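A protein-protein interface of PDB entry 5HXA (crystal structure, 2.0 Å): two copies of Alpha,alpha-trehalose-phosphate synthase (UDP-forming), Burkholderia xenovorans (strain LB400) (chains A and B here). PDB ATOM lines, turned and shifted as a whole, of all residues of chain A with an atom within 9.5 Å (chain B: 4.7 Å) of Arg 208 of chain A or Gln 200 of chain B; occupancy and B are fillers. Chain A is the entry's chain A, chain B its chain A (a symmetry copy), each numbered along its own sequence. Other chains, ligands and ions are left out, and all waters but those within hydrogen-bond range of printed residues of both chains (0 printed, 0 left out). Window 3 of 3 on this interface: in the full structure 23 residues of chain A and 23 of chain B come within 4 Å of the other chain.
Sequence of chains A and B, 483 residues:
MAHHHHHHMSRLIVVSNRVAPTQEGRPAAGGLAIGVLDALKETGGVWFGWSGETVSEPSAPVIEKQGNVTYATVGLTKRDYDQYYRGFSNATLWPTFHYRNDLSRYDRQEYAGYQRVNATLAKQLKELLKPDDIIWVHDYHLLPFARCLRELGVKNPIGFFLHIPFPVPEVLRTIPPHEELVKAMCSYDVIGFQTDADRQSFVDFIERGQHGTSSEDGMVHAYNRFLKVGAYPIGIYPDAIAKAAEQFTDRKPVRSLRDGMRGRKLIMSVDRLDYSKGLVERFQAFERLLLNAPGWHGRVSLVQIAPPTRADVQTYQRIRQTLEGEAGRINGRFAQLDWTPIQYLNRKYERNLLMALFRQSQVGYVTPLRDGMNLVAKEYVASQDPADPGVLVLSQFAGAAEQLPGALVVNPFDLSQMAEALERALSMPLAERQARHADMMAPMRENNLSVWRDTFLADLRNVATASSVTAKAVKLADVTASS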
ATOM      1  N   VAL A 168      10.882 -34.847 -31.039  1.00  0.00           N
ATOM      2  CA  VAL A 168      10.190 -34.127 -29.965  1.00  0.00           C
ATOM      3  C   VAL A 168      11.123 -34.005 -28.763  1.00  0.00           C
ATOM      4  O   VAL A 168      12.119 -34.746 -28.680  1.00  0.00           O
ATOM      5  CB  VAL A 168       8.862 -34.817 -29.597  1.00  0.00           C
ATOM      6  CG1 VAL A 168       7.853 -34.706 -30.768  1.00  0.00           C
ATOM      7  CG2 VAL A 168       9.092 -36.251 -29.223  1.00  0.00           C
ATOM      8  N   PRO A 169      10.857 -33.081 -27.831  1.00  0.00           N
ATOM      9  CA  PRO A 169      11.810 -32.835 -26.731  1.00  0.00           C
ATOM     10  C   PRO A 169      12.210 -34.063 -25.922  1.00  0.00           C
ATOM     11  O   PRO A 169      13.394 -34.187 -25.586  1.00  0.00           O
ATOM     12  CB  PRO A 169      11.059 -31.807 -25.863  1.00  0.00           C
ATOM     13  CG  PRO A 169      10.280 -31.001 -26.876  1.00  0.00           C
ATOM     14  CD  PRO A 169       9.813 -32.035 -27.894  1.00  0.00           C
ATOM     15  N   GLU A 170      11.277 -34.959 -25.575  1.00  0.00           N
ATOM     16  CA  GLU A 170      11.652 -36.134 -24.782  1.00  0.00           C
ATOM     17  C   GLU A 170      12.743 -36.952 -25.457  1.00  0.00           C
ATOM     18  O   GLU A 170      13.512 -37.635 -24.771  1.00  0.00           O
ATOM     19  CB  GLU A 170      10.440 -37.032 -24.518  1.00  0.00           C
ATOM     20  CG  GLU A 170       9.485 -36.511 -23.441  1.00  0.00           C
ATOM     21  CD  GLU A 170      10.125 -36.463 -22.058  1.00  0.00           C
ATOM     22  OE1 GLU A 170      11.118 -37.193 -21.785  1.00  0.00           O
ATOM     23  OE2 GLU A 170       9.605 -35.706 -21.225  1.00  0.00           O
ATOM     24  N   GLU A 179      20.960 -28.731 -25.783  1.00  0.00           N
ATOM     25  CA  GLU A 179      20.619 -27.333 -25.500  1.00  0.00           C
ATOM     26  C   GLU A 179      21.497 -26.366 -26.288  1.00  0.00           C
ATOM     27  O   GLU A 179      21.009 -25.354 -26.815  1.00  0.00           O
ATOM     28  CB  GLU A 179      20.716 -27.060 -24.001  1.00  0.00           C
ATOM     29  CG  GLU A 179      19.822 -27.970 -23.203  1.00  0.00           C
ATOM     30  CD  GLU A 179      19.363 -27.350 -21.908  1.00  0.00           C
ATOM     31  OE1 GLU A 179      18.142 -27.389 -21.633  1.00  0.00           O
ATOM     32  OE2 GLU A 179      20.223 -26.815 -21.177  1.00  0.00           O
ATOM     33  N   GLN A 200       6.541 -27.962 -34.926  1.00  0.00           N
ATOM     34  CA  GLN A 200       5.996 -27.894 -33.575  1.00  0.00           C
ATOM     35  C   GLN A 200       6.948 -28.520 -32.562  1.00  0.00           C
ATOM     36  O   GLN A 200       7.067 -28.019 -31.439  1.00  0.00           O
ATOM     37  CB  GLN A 200       4.621 -28.562 -33.517  1.00  0.00           C
ATOM     38  CG  GLN A 200       3.864 -28.302 -32.206  1.00  0.00           C
ATOM     39  CD  GLN A 200       3.629 -26.821 -31.945  1.00  0.00           C
ATOM     40  OE1 GLN A 200       3.104 -26.103 -32.797  1.00  0.00           O
ATOM     41  NE2 GLN A 200       4.031 -26.353 -30.761  1.00  0.00           N
ATOM     42  N   SER A 201       7.646 -29.594 -32.947  1.00  0.00           N
ATOM     43  CA  SER A 201       8.647 -30.203 -32.078  1.00  0.00           C
ATOM     44  C   SER A 201       9.724 -29.199 -31.678  1.00  0.00           C
ATOM     45  O   SER A 201      10.126 -29.128 -30.509  1.00  0.00           O
ATOM     46  CB  SER A 201       9.270 -31.394 -32.804  1.00  0.00           C
ATOM     47  OG  SER A 201      10.431 -31.830 -32.147  1.00  0.00           O
ATOM     48  N   PHE A 202      10.224 -28.434 -32.650  1.00  0.00           N
ATOM     49  CA  PHE A 202      11.257 -27.434 -32.381  1.00  0.00           C
ATOM     50  C   PHE A 202      10.717 -26.336 -31.476  1.00  0.00           C
ATOM     51  O   PHE A 202      11.343 -25.966 -30.479  1.00  0.00           O
ATOM     52  CB  PHE A 202      11.745 -26.852 -33.708  1.00  0.00           C
ATOM     53  CG  PHE A 202      12.812 -25.796 -33.578  1.00  0.00           C
ATOM     54  CD1 PHE A 202      14.140 -26.149 -33.372  1.00  0.00           C
ATOM     55  CD2 PHE A 202      12.491 -24.453 -33.704  1.00  0.00           C
ATOM     56  CE1 PHE A 202      15.130 -25.167 -33.276  1.00  0.00           C
ATOM     57  CE2 PHE A 202      13.473 -23.475 -33.611  1.00  0.00           C
ATOM     58  CZ  PHE A 202      14.791 -23.829 -33.397  1.00  0.00           C
ATOM     59  N   VAL A 203       9.544 -25.805 -31.814  1.00  0.00           N
ATOM     60  CA  VAL A 203       8.964 -24.730 -31.020  1.00  0.00           C
ATOM     61  C   VAL A 203       8.603 -25.226 -29.621  1.00  0.00           C
ATOM     62  O   VAL A 203       8.763 -24.498 -28.629  1.00  0.00           O
ATOM     63  CB  VAL A 203       7.748 -24.142 -31.757  1.00  0.00           C
ATOM     64  CG1 VAL A 203       7.000 -23.169 -30.860  1.00  0.00           C
ATOM     65  CG2 VAL A 203       8.202 -23.455 -33.059  1.00  0.00           C
ATOM     66  N   ASP A 204       8.130 -26.475 -29.512  1.00  0.00           N
ATOM     67  CA  ASP A 204       7.850 -27.042 -28.189  1.00  0.00           C
ATOM     68  C   ASP A 204       9.090 -27.037 -27.303  1.00  0.00           C
ATOM     69  O   ASP A 204       9.007 -26.748 -26.100  1.00  0.00           O
ATOM     70  CB  ASP A 204       7.327 -28.473 -28.312  1.00  0.00           C
ATOM     71  CG  ASP A 204       5.837 -28.543 -28.629  1.00  0.00           C
ATOM     72  OD1 ASP A 204       5.147 -27.503 -28.568  1.00  0.00           O
ATOM     73  OD2 ASP A 204       5.357 -29.657 -28.928  1.00  0.00           O
ATOM     74  N   PHE A 205      10.246 -27.398 -27.859  1.00  0.00           N
ATOM     75  CA  PHE A 205      11.446 -27.415 -27.030  1.00  0.00           C
ATOM     76  C   PHE A 205      11.720 -26.025 -26.485  1.00  0.00           C
ATOM     77  O   PHE A 205      11.989 -25.843 -25.288  1.00  0.00           O
ATOM     78  CB  PHE A 205      12.661 -27.917 -27.817  1.00  0.00           C
ATOM     79  CG  PHE A 205      13.925 -27.884 -27.003  1.00  0.00           C
ATOM     80  CD1 PHE A 205      14.263 -28.954 -26.181  1.00  0.00           C
ATOM     81  CD2 PHE A 205      14.730 -26.743 -26.984  1.00  0.00           C
ATOM     82  CE1 PHE A 205      15.409 -28.907 -25.382  1.00  0.00           C
ATOM     83  CE2 PHE A 205      15.869 -26.692 -26.202  1.00  0.00           C
ATOM     84  CZ  PHE A 205      16.213 -27.776 -25.401  1.00  0.00           C
ATOM     85  N   ILE A 206      11.631 -25.031 -27.363  1.00  0.00           N
ATOM     86  CA  ILE A 206      11.963 -23.659 -26.996  1.00  0.00           C
ATOM     87  C   ILE A 206      10.991 -23.135 -25.949  1.00  0.00           C
ATOM     88  O   ILE A 206      11.400 -22.559 -24.933  1.00  0.00           O
ATOM     89  CB  ILE A 206      11.990 -22.787 -28.267  1.00  0.00           C
ATOM     90  CG1 ILE A 206      13.267 -23.108 -29.055  1.00  0.00           C
ATOM     91  CG2 ILE A 206      11.874 -21.279 -27.950  1.00  0.00           C
ATOM     92  CD1 ILE A 206      13.322 -22.480 -30.396  1.00  0.00           C
ATOM     93  N   GLU A 207       9.690 -23.340 -26.169  1.00  0.00           N
ATOM     94  CA  GLU A 207       8.702 -22.803 -25.238  1.00  0.00           C
ATOM     95  C   GLU A 207       8.732 -23.544 -23.910  1.00  0.00           C
ATOM     96  O   GLU A 207       8.702 -22.926 -22.841  1.00  0.00           O
ATOM     97  CB  GLU A 207       7.299 -22.874 -25.850  1.00  0.00           C
ATOM     98  CG  GLU A 207       7.091 -21.941 -27.030  1.00  0.00           C
ATOM     99  CD  GLU A 207       5.660 -21.969 -27.553  1.00  0.00           C
ATOM    100  OE1 GLU A 207       5.183 -20.932 -28.039  1.00  0.00           O
ATOM    101  OE2 GLU A 207       5.012 -23.032 -27.472  1.00  0.00           O
ATOM    102  N   ARG A 208       8.777 -24.876 -23.951  1.00  0.00           N
ATOM    103  CA  ARG A 208       8.674 -25.634 -22.709  1.00  0.00           C
ATOM    104  C   ARG A 208       9.954 -25.571 -21.895  1.00  0.00           C
ATOM    105  O   ARG A 208       9.902 -25.713 -20.670  1.00  0.00           O
ATOM    106  CB  ARG A 208       8.259 -27.079 -23.022  1.00  0.00           C
ATOM    107  CG  ARG A 208       6.872 -27.080 -23.646  1.00  0.00           C
ATOM    108  CD  ARG A 208       6.322 -28.437 -24.082  1.00  0.00           C
ATOM    109  NE  ARG A 208       4.888 -28.271 -24.335  1.00  0.00           N
ATOM    110  CZ  ARG A 208       4.061 -29.220 -24.767  1.00  0.00           C
ATOM    111  NH1 ARG A 208       4.513 -30.435 -25.011  1.00  0.00           N
ATOM    112  NH2 ARG A 208       2.773 -28.944 -24.951  1.00  0.00           N
ATOM    113  N   GLY A 209      11.089 -25.320 -22.535  1.00  0.00           N
ATOM    114  CA  GLY A 209      12.308 -25.044 -21.800  1.00  0.00           C
ATOM    115  C   GLY A 209      12.475 -23.601 -21.377  1.00  0.00           C
ATOM    116  O   GLY A 209      13.526 -23.247 -20.838  1.00  0.00           O
ATOM    117  N   GLN A 210      11.458 -22.764 -21.615  1.00  0.00           N
ATOM    118  CA  GLN A 210      11.488 -21.333 -21.279  1.00  0.00           C
ATOM    119  C   GLN A 210      12.654 -20.616 -21.954  1.00  0.00           C
ATOM    120  O   GLN A 210      13.243 -19.689 -21.394  1.00  0.00           O
ATOM    121  CB  GLN A 210      11.523 -21.099 -19.766  1.00  0.00           C
ATOM    122  CG  GLN A 210      10.194 -21.341 -19.083  1.00  0.00           C
ATOM    123  CD  GLN A 210       9.887 -22.811 -18.953  1.00  0.00           C
ATOM    124  OE1 GLN A 210      10.742 -23.594 -18.539  1.00  0.00           O
ATOM    125  NE2 GLN A 210       8.669 -23.200 -19.318  1.00  0.00           N
ATOM    126  N   HIS A 211      12.985 -21.038 -23.174  1.00  0.00           N
ATOM    127  CA  HIS A 211      14.039 -20.391 -23.945  1.00  0.00           C
ATOM    128  C   HIS A 211      13.518 -19.288 -24.846  1.00  0.00           C
ATOM    129  O   HIS A 211      14.311 -18.474 -25.336  1.00  0.00           O
ATOM    130  CB  HIS A 211      14.772 -21.417 -24.817  1.00  0.00           C
ATOM    131  CG  HIS A 211      15.365 -22.542 -24.040  1.00  0.00           C
ATOM    132  ND1 HIS A 211      16.360 -22.351 -23.107  1.00  0.00           N
ATOM    133  CD2 HIS A 211      15.098 -23.867 -24.044  1.00  0.00           C
ATOM    134  CE1 HIS A 211      16.684 -23.515 -22.572  1.00  0.00           C
ATOM    135  NE2 HIS A 211      15.931 -24.450 -23.121  1.00  0.00           N
ATOM    136  N   GLY A 212      12.217 -19.258 -25.100  1.00  0.00           N
ATOM    137  CA  GLY A 212      11.674 -18.267 -26.006  1.00  0.00           C
ATOM    138  C   GLY A 212      10.183 -18.453 -26.132  1.00  0.00           C
ATOM    139  O   GLY A 212       9.579 -19.295 -25.462  1.00  0.00           O
ATOM    140  N   THR A 213       9.590 -17.655 -27.016  1.00  0.00           N
ATOM    141  CA  THR A 213       8.144 -17.633 -27.176  1.00  0.00           C
ATOM    142  C   THR A 213       7.808 -17.618 -28.660  1.00  0.00           C
ATOM    143  O   THR A 213       8.625 -17.236 -29.498  1.00  0.00           O
ATOM    144  CB  THR A 213       7.517 -16.403 -26.484  1.00  0.00           C
ATOM    145  OG1 THR A 213       8.144 -15.213 -26.983  1.00  0.00           O
ATOM    146  CG2 THR A 213       7.719 -16.458 -24.965  1.00  0.00           C
ATOM    147  N   SER A 214       6.586 -18.037 -28.976  1.00  0.00           N
ATOM    148  CA  SER A 214       6.041 -17.908 -30.321  1.00  0.00           C
ATOM    149  C   SER A 214       5.446 -16.524 -30.506  1.00  0.00           C
ATOM    150  O   SER A 214       4.886 -15.942 -29.572  1.00  0.00           O
ATOM    151  CB  SER A 214       4.959 -18.956 -30.584  1.00  0.00           C
ATOM    152  OG  SER A 214       5.538 -20.188 -30.937  1.00  0.00           O
ATOM    153  N   TYR A 223      16.534 -16.767 -27.365  1.00  0.00           N
ATOM    154  CA  TYR A 223      17.968 -16.507 -27.221  1.00  0.00           C
ATOM    155  C   TYR A 223      18.336 -15.123 -27.756  1.00  0.00           C
ATOM    156  O   TYR A 223      19.335 -14.951 -28.467  1.00  0.00           O
ATOM    157  CB  TYR A 223      18.799 -17.595 -27.910  1.00  0.00           C
ATOM    158  CG  TYR A 223      18.362 -19.014 -27.584  1.00  0.00           C
ATOM    159  CD1 TYR A 223      18.796 -19.648 -26.426  1.00  0.00           C
ATOM    160  CD2 TYR A 223      17.517 -19.711 -28.437  1.00  0.00           C
ATOM    161  CE1 TYR A 223      18.389 -20.956 -26.131  1.00  0.00           C
ATOM    162  CE2 TYR A 223      17.109 -21.011 -28.150  1.00  0.00           C
ATOM    163  CZ  TYR A 223      17.552 -21.624 -26.993  1.00  0.00           C
ATOM    164  OH  TYR A 223      17.155 -22.911 -26.700  1.00  0.00           O
ATOM    165  N   ASP B 196       4.655 -34.408 -14.276  1.00  0.00           N
ATOM    166  CA  ASP B 196       3.962 -33.433 -15.120  1.00  0.00           C
ATOM    167  C   ASP B 196       4.171 -33.735 -16.598  1.00  0.00           C
ATOM    168  O   ASP B 196       3.276 -33.509 -17.420  1.00  0.00           O
ATOM    169  CB  ASP B 196       4.457 -32.010 -14.823  1.00  0.00           C
ATOM    170  CG  ASP B 196       4.191 -31.562 -13.395  1.00  0.00           C
ATOM    171  OD1 ASP B 196       3.147 -31.927 -12.826  1.00  0.00           O
ATOM    172  OD2 ASP B 196       5.030 -30.812 -12.851  1.00  0.00           O
ATOM    173  N   ALA B 197       5.366 -34.220 -16.962  1.00  0.00           N
ATOM    174  CA  ALA B 197       5.623 -34.534 -18.369  1.00  0.00           C
ATOM    175  C   ALA B 197       4.706 -35.652 -18.859  1.00  0.00           C
ATOM    176  O   ALA B 197       4.243 -35.624 -20.004  1.00  0.00           O
ATOM    177  CB  ALA B 197       7.094 -34.920 -18.575  1.00  0.00           C
ATOM    178  N   ASP B 198       4.434 -36.647 -18.006  1.00  0.00           N
ATOM    179  CA  ASP B 198       3.486 -37.697 -18.378  1.00  0.00           C
ATOM    180  C   ASP B 198       2.083 -37.133 -18.544  1.00  0.00           C
ATOM    181  O   ASP B 198       1.369 -37.498 -19.490  1.00  0.00           O
ATOM    182  CB  ASP B 198       3.478 -38.811 -17.332  1.00  0.00           C
ATOM    183  CG  ASP B 198       4.838 -39.453 -17.161  1.00  0.00           C
ATOM    184  OD1 ASP B 198       5.416 -39.873 -18.183  1.00  0.00           O
ATOM    185  OD2 ASP B 198       5.330 -39.524 -16.013  1.00  0.00           O
ATOM    186  N   ARG B 199       1.661 -36.257 -17.623  1.00  0.00           N
ATOM    187  CA  ARG B 199       0.344 -35.637 -17.746  1.00  0.00           C
ATOM    188  C   ARG B 199       0.246 -34.824 -19.029  1.00  0.00           C
ATOM    189  O   ARG B 199      -0.755 -34.900 -19.753  1.00  0.00           O
ATOM    190  CB  ARG B 199       0.054 -34.742 -16.536  1.00  0.00           C
ATOM    191  CG  ARG B 199      -1.286 -33.993 -16.656  1.00  0.00           C
ATOM    192  CD  ARG B 199      -1.277 -32.663 -15.919  1.00  0.00           C
ATOM    193  NE  ARG B 199      -0.050 -31.917 -16.172  1.00  0.00           N
ATOM    194  CZ  ARG B 199       0.179 -31.179 -17.255  1.00  0.00           C
ATOM    195  NH1 ARG B 199      -0.739 -31.070 -18.204  1.00  0.00           N
ATOM    196  NH2 ARG B 199       1.340 -30.560 -17.389  1.00  0.00           N
ATOM    197  N   GLN B 200       1.277 -34.022 -19.315  1.00  0.00           N
ATOM    198  CA  GLN B 200       1.239 -33.194 -20.514  1.00  0.00           C
ATOM    199  C   GLN B 200       1.248 -34.047 -21.777  1.00  0.00           C
ATOM    200  O   GLN B 200       0.579 -33.703 -22.757  1.00  0.00           O
ATOM    201  CB  GLN B 200       2.403 -32.202 -20.518  1.00  0.00           C
ATOM    202  CG  GLN B 200       2.288 -31.119 -21.601  1.00  0.00           C
ATOM    203  CD  GLN B 200       1.020 -30.287 -21.471  1.00  0.00           C
ATOM    204  OE1 GLN B 200       0.726 -29.744 -20.406  1.00  0.00           O
ATOM    205  NE2 GLN B 200       0.254 -30.194 -22.560  1.00  0.00           N
ATOM    206  N   SER B 201       1.976 -35.169 -21.764  1.00  0.00           N
ATOM    207  CA  SER B 201       1.972 -36.094 -22.892  1.00  0.00           C
ATOM    208  C   SER B 201       0.561 -36.585 -23.205  1.00  0.00           C
ATOM    209  O   SER B 201       0.153 -36.646 -24.373  1.00  0.00           O
ATOM    210  CB  SER B 201       2.888 -37.272 -22.566  1.00  0.00           C
ATOM    211  OG  SER B 201       2.694 -38.324 -23.475  1.00  0.00           O
ATOM    212  N   PHE B 202      -0.186 -36.970 -22.169  1.00  0.00           N
ATOM    213  CA  PHE B 202      -1.554 -37.453 -22.351  1.00  0.00           C
ATOM    214  C   PHE B 202      -2.449 -36.343 -22.882  1.00  0.00           C
ATOM    215  O   PHE B 202      -3.193 -36.532 -23.848  1.00  0.00           O
ATOM    216  CB  PHE B 202      -2.078 -37.980 -21.014  1.00  0.00           C
ATOM    217  CG  PHE B 202      -3.489 -38.505 -21.055  1.00  0.00           C
ATOM    218  CD1 PHE B 202      -3.760 -39.781 -21.536  1.00  0.00           C
ATOM    219  CD2 PHE B 202      -4.539 -37.739 -20.572  1.00  0.00           C
ATOM    220  CE1 PHE B 202      -5.068 -40.273 -21.549  1.00  0.00           C
ATOM    221  CE2 PHE B 202      -5.840 -38.226 -20.582  1.00  0.00           C
ATOM    222  CZ  PHE B 202      -6.106 -39.491 -21.070  1.00  0.00           C
ATOM    223  N   VAL B 203      -2.383 -35.170 -22.256  1.00  0.00           N
ATOM    224  CA  VAL B 203      -3.224 -34.059 -22.680  1.00  0.00           C
ATOM    225  C   VAL B 203      -2.840 -33.597 -24.085  1.00  0.00           C
ATOM    226  O   VAL B 203      -3.709 -33.233 -24.892  1.00  0.00           O
ATOM    227  CB  VAL B 203      -3.130 -32.918 -21.651  1.00  0.00           C
ATOM    228  CG1 VAL B 203      -3.825 -31.671 -22.172  1.00  0.00           C
ATOM    229  CG2 VAL B 203      -3.738 -33.369 -20.309  1.00  0.00           C
ATOM    230  N   ASP B 204      -1.541 -33.620 -24.409  1.00  0.00           N
ATOM    231  CA  ASP B 204      -1.116 -33.276 -25.770  1.00  0.00           C
ATOM    232  C   ASP B 204      -1.773 -34.179 -26.807  1.00  0.00           C
ATOM    233  O   ASP B 204      -2.179 -33.714 -27.883  1.00  0.00           O
ATOM    234  CB  ASP B 204       0.404 -33.379 -25.906  1.00  0.00           C
ATOM    235  CG  ASP B 204       1.137 -32.144 -25.392  1.00  0.00           C
ATOM    236  OD1 ASP B 204       0.485 -31.118 -25.104  1.00  0.00           O
ATOM    237  OD2 ASP B 204       2.380 -32.205 -25.292  1.00  0.00           O
ATOM    238  N   ARG B 208      -4.085 -32.298 -29.476  1.00  0.00           N
ATOM    239  CA  ARG B 208      -3.551 -32.203 -30.830  1.00  0.00           C
ATOM    240  C   ARG B 208      -4.267 -33.136 -31.791  1.00  0.00           C
ATOM    241  O   ARG B 208      -4.303 -32.857 -32.993  1.00  0.00           O
ATOM    242  CB  ARG B 208      -2.036 -32.451 -30.804  1.00  0.00           C
ATOM    243  CG  ARG B 208      -1.361 -31.355 -29.994  1.00  0.00           C
ATOM    244  CD  ARG B 208       0.151 -31.478 -29.809  1.00  0.00           C
ATOM    245  NE  ARG B 208       0.640 -30.190 -29.309  1.00  0.00           N
ATOM    246  CZ  ARG B 208       1.901 -29.909 -28.991  1.00  0.00           C
ATOM    247  NH1 ARG B 208       2.837 -30.831 -29.108  1.00  0.00           N
ATOM    248  NH2 ARG B 208       2.220 -28.694 -28.554  1.00  0.00           N
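OD2 of Asp 204 of chain A is in salt-bridge range of NH1 of Arg 208 of chain B (2.8 Å). The guanidinium group (NH1) of Arg 208 of chain A is in salt-bridge range of the side-chain carboxylate (OD2) of Asp 204 of chain B (2.8 Å).
OD1 of Asp 204 of chain B lies within hydrogen-bond range of NE2 of Gln 200 of chain B (2.7 Å). The backbone carbonyl oxygen of Arg 208 of chain A sits at hydrogen-bond distance from the side-chain amide nitrogen of Gln 210 of chain A, at 3.1 Å. The guanidinium group of Arg 199 of chain B sits at hydrogen-bond distance from the side-chain amide oxygen of Gln 200 of chain B. The side-chain amide nitrogen (NE2) of Gln 200 of chain A sits at hydrogen-bond distance from the side-chain carboxylate (OD1) of Asp 204 of chain A (2.7 Å).
Among the printed residues, merely in contact across the chains: Arg 208 of chain A with Arg 208 of chain B (3.7 Å), Arg 208 of chain A with Gln 200 of chain B (3.7 Å), Gln 200 of chain A with Arg 208 of chain B (3.7 Å) and Glu 170 of chain A with Ala 197 of chain B (3.7 Å).
Of the printed residues of chain B, Glu 170 of chain A touches Ala 197 (3.7 Å). Printed residues of chain B within 4 Å of Gln 200 of chain A: Arg 208. Of the printed residues of chain B, Asp 204 of chain A touches Arg 208 (2.8 Å). Printed residues of chain B within 4 Å of Arg 208 of chain A: Gln 200, Asp 204 and Arg 208. Printed residues of chain A within 4 Å of Ala 197 of chain B: Glu 170. Of the printed residues of chain A, Gln 200 of chain B touches Arg 208. Val 203 of chain B touches none of the printed residues of chain A. Printed residues of chain A within 4 Å of Asp 204 of chain B: Arg 208 (2.8 Å). The nearest printed residue of chain B that does not touch Arg 208 of chain A is Ser 201 of chain B (6.3 Å).
Of the 20 printed residues of chain A, 4 touch a printed residue of chain B. Of the 10 printed residues of chain B, 4 touch a printed residue of chain A. Hydrophobic or aromatic side chains of chain B within 4 Å of the printed part of chain A: Ala 197. Along chain B the printed residues that touch a printed residue of chain A span positions 197 to 208. Among the printed residues, 6 pairs touch across the chains. Among the printed residues, Asp or Glu carboxylates within 4 Å of a Lys or Arg side-chain nitrogen of the other chain: Asp 204 of chain A with Arg 208 of chain B and Arg 208 of chain A with Asp 204 of chain B.
Gln 200 of chain A touches Arg 208 of chain B, and with the chains exchanged Arg 208 of chain A touches Gln 200 of chain B. Asp 204 of chain A touches Arg 208 of chain B, and with the chains exchanged Arg 208 of chain A touches Asp 204 of chain B. Arg 208 of chain B touches its own counterpart, Arg 208 of chain A.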
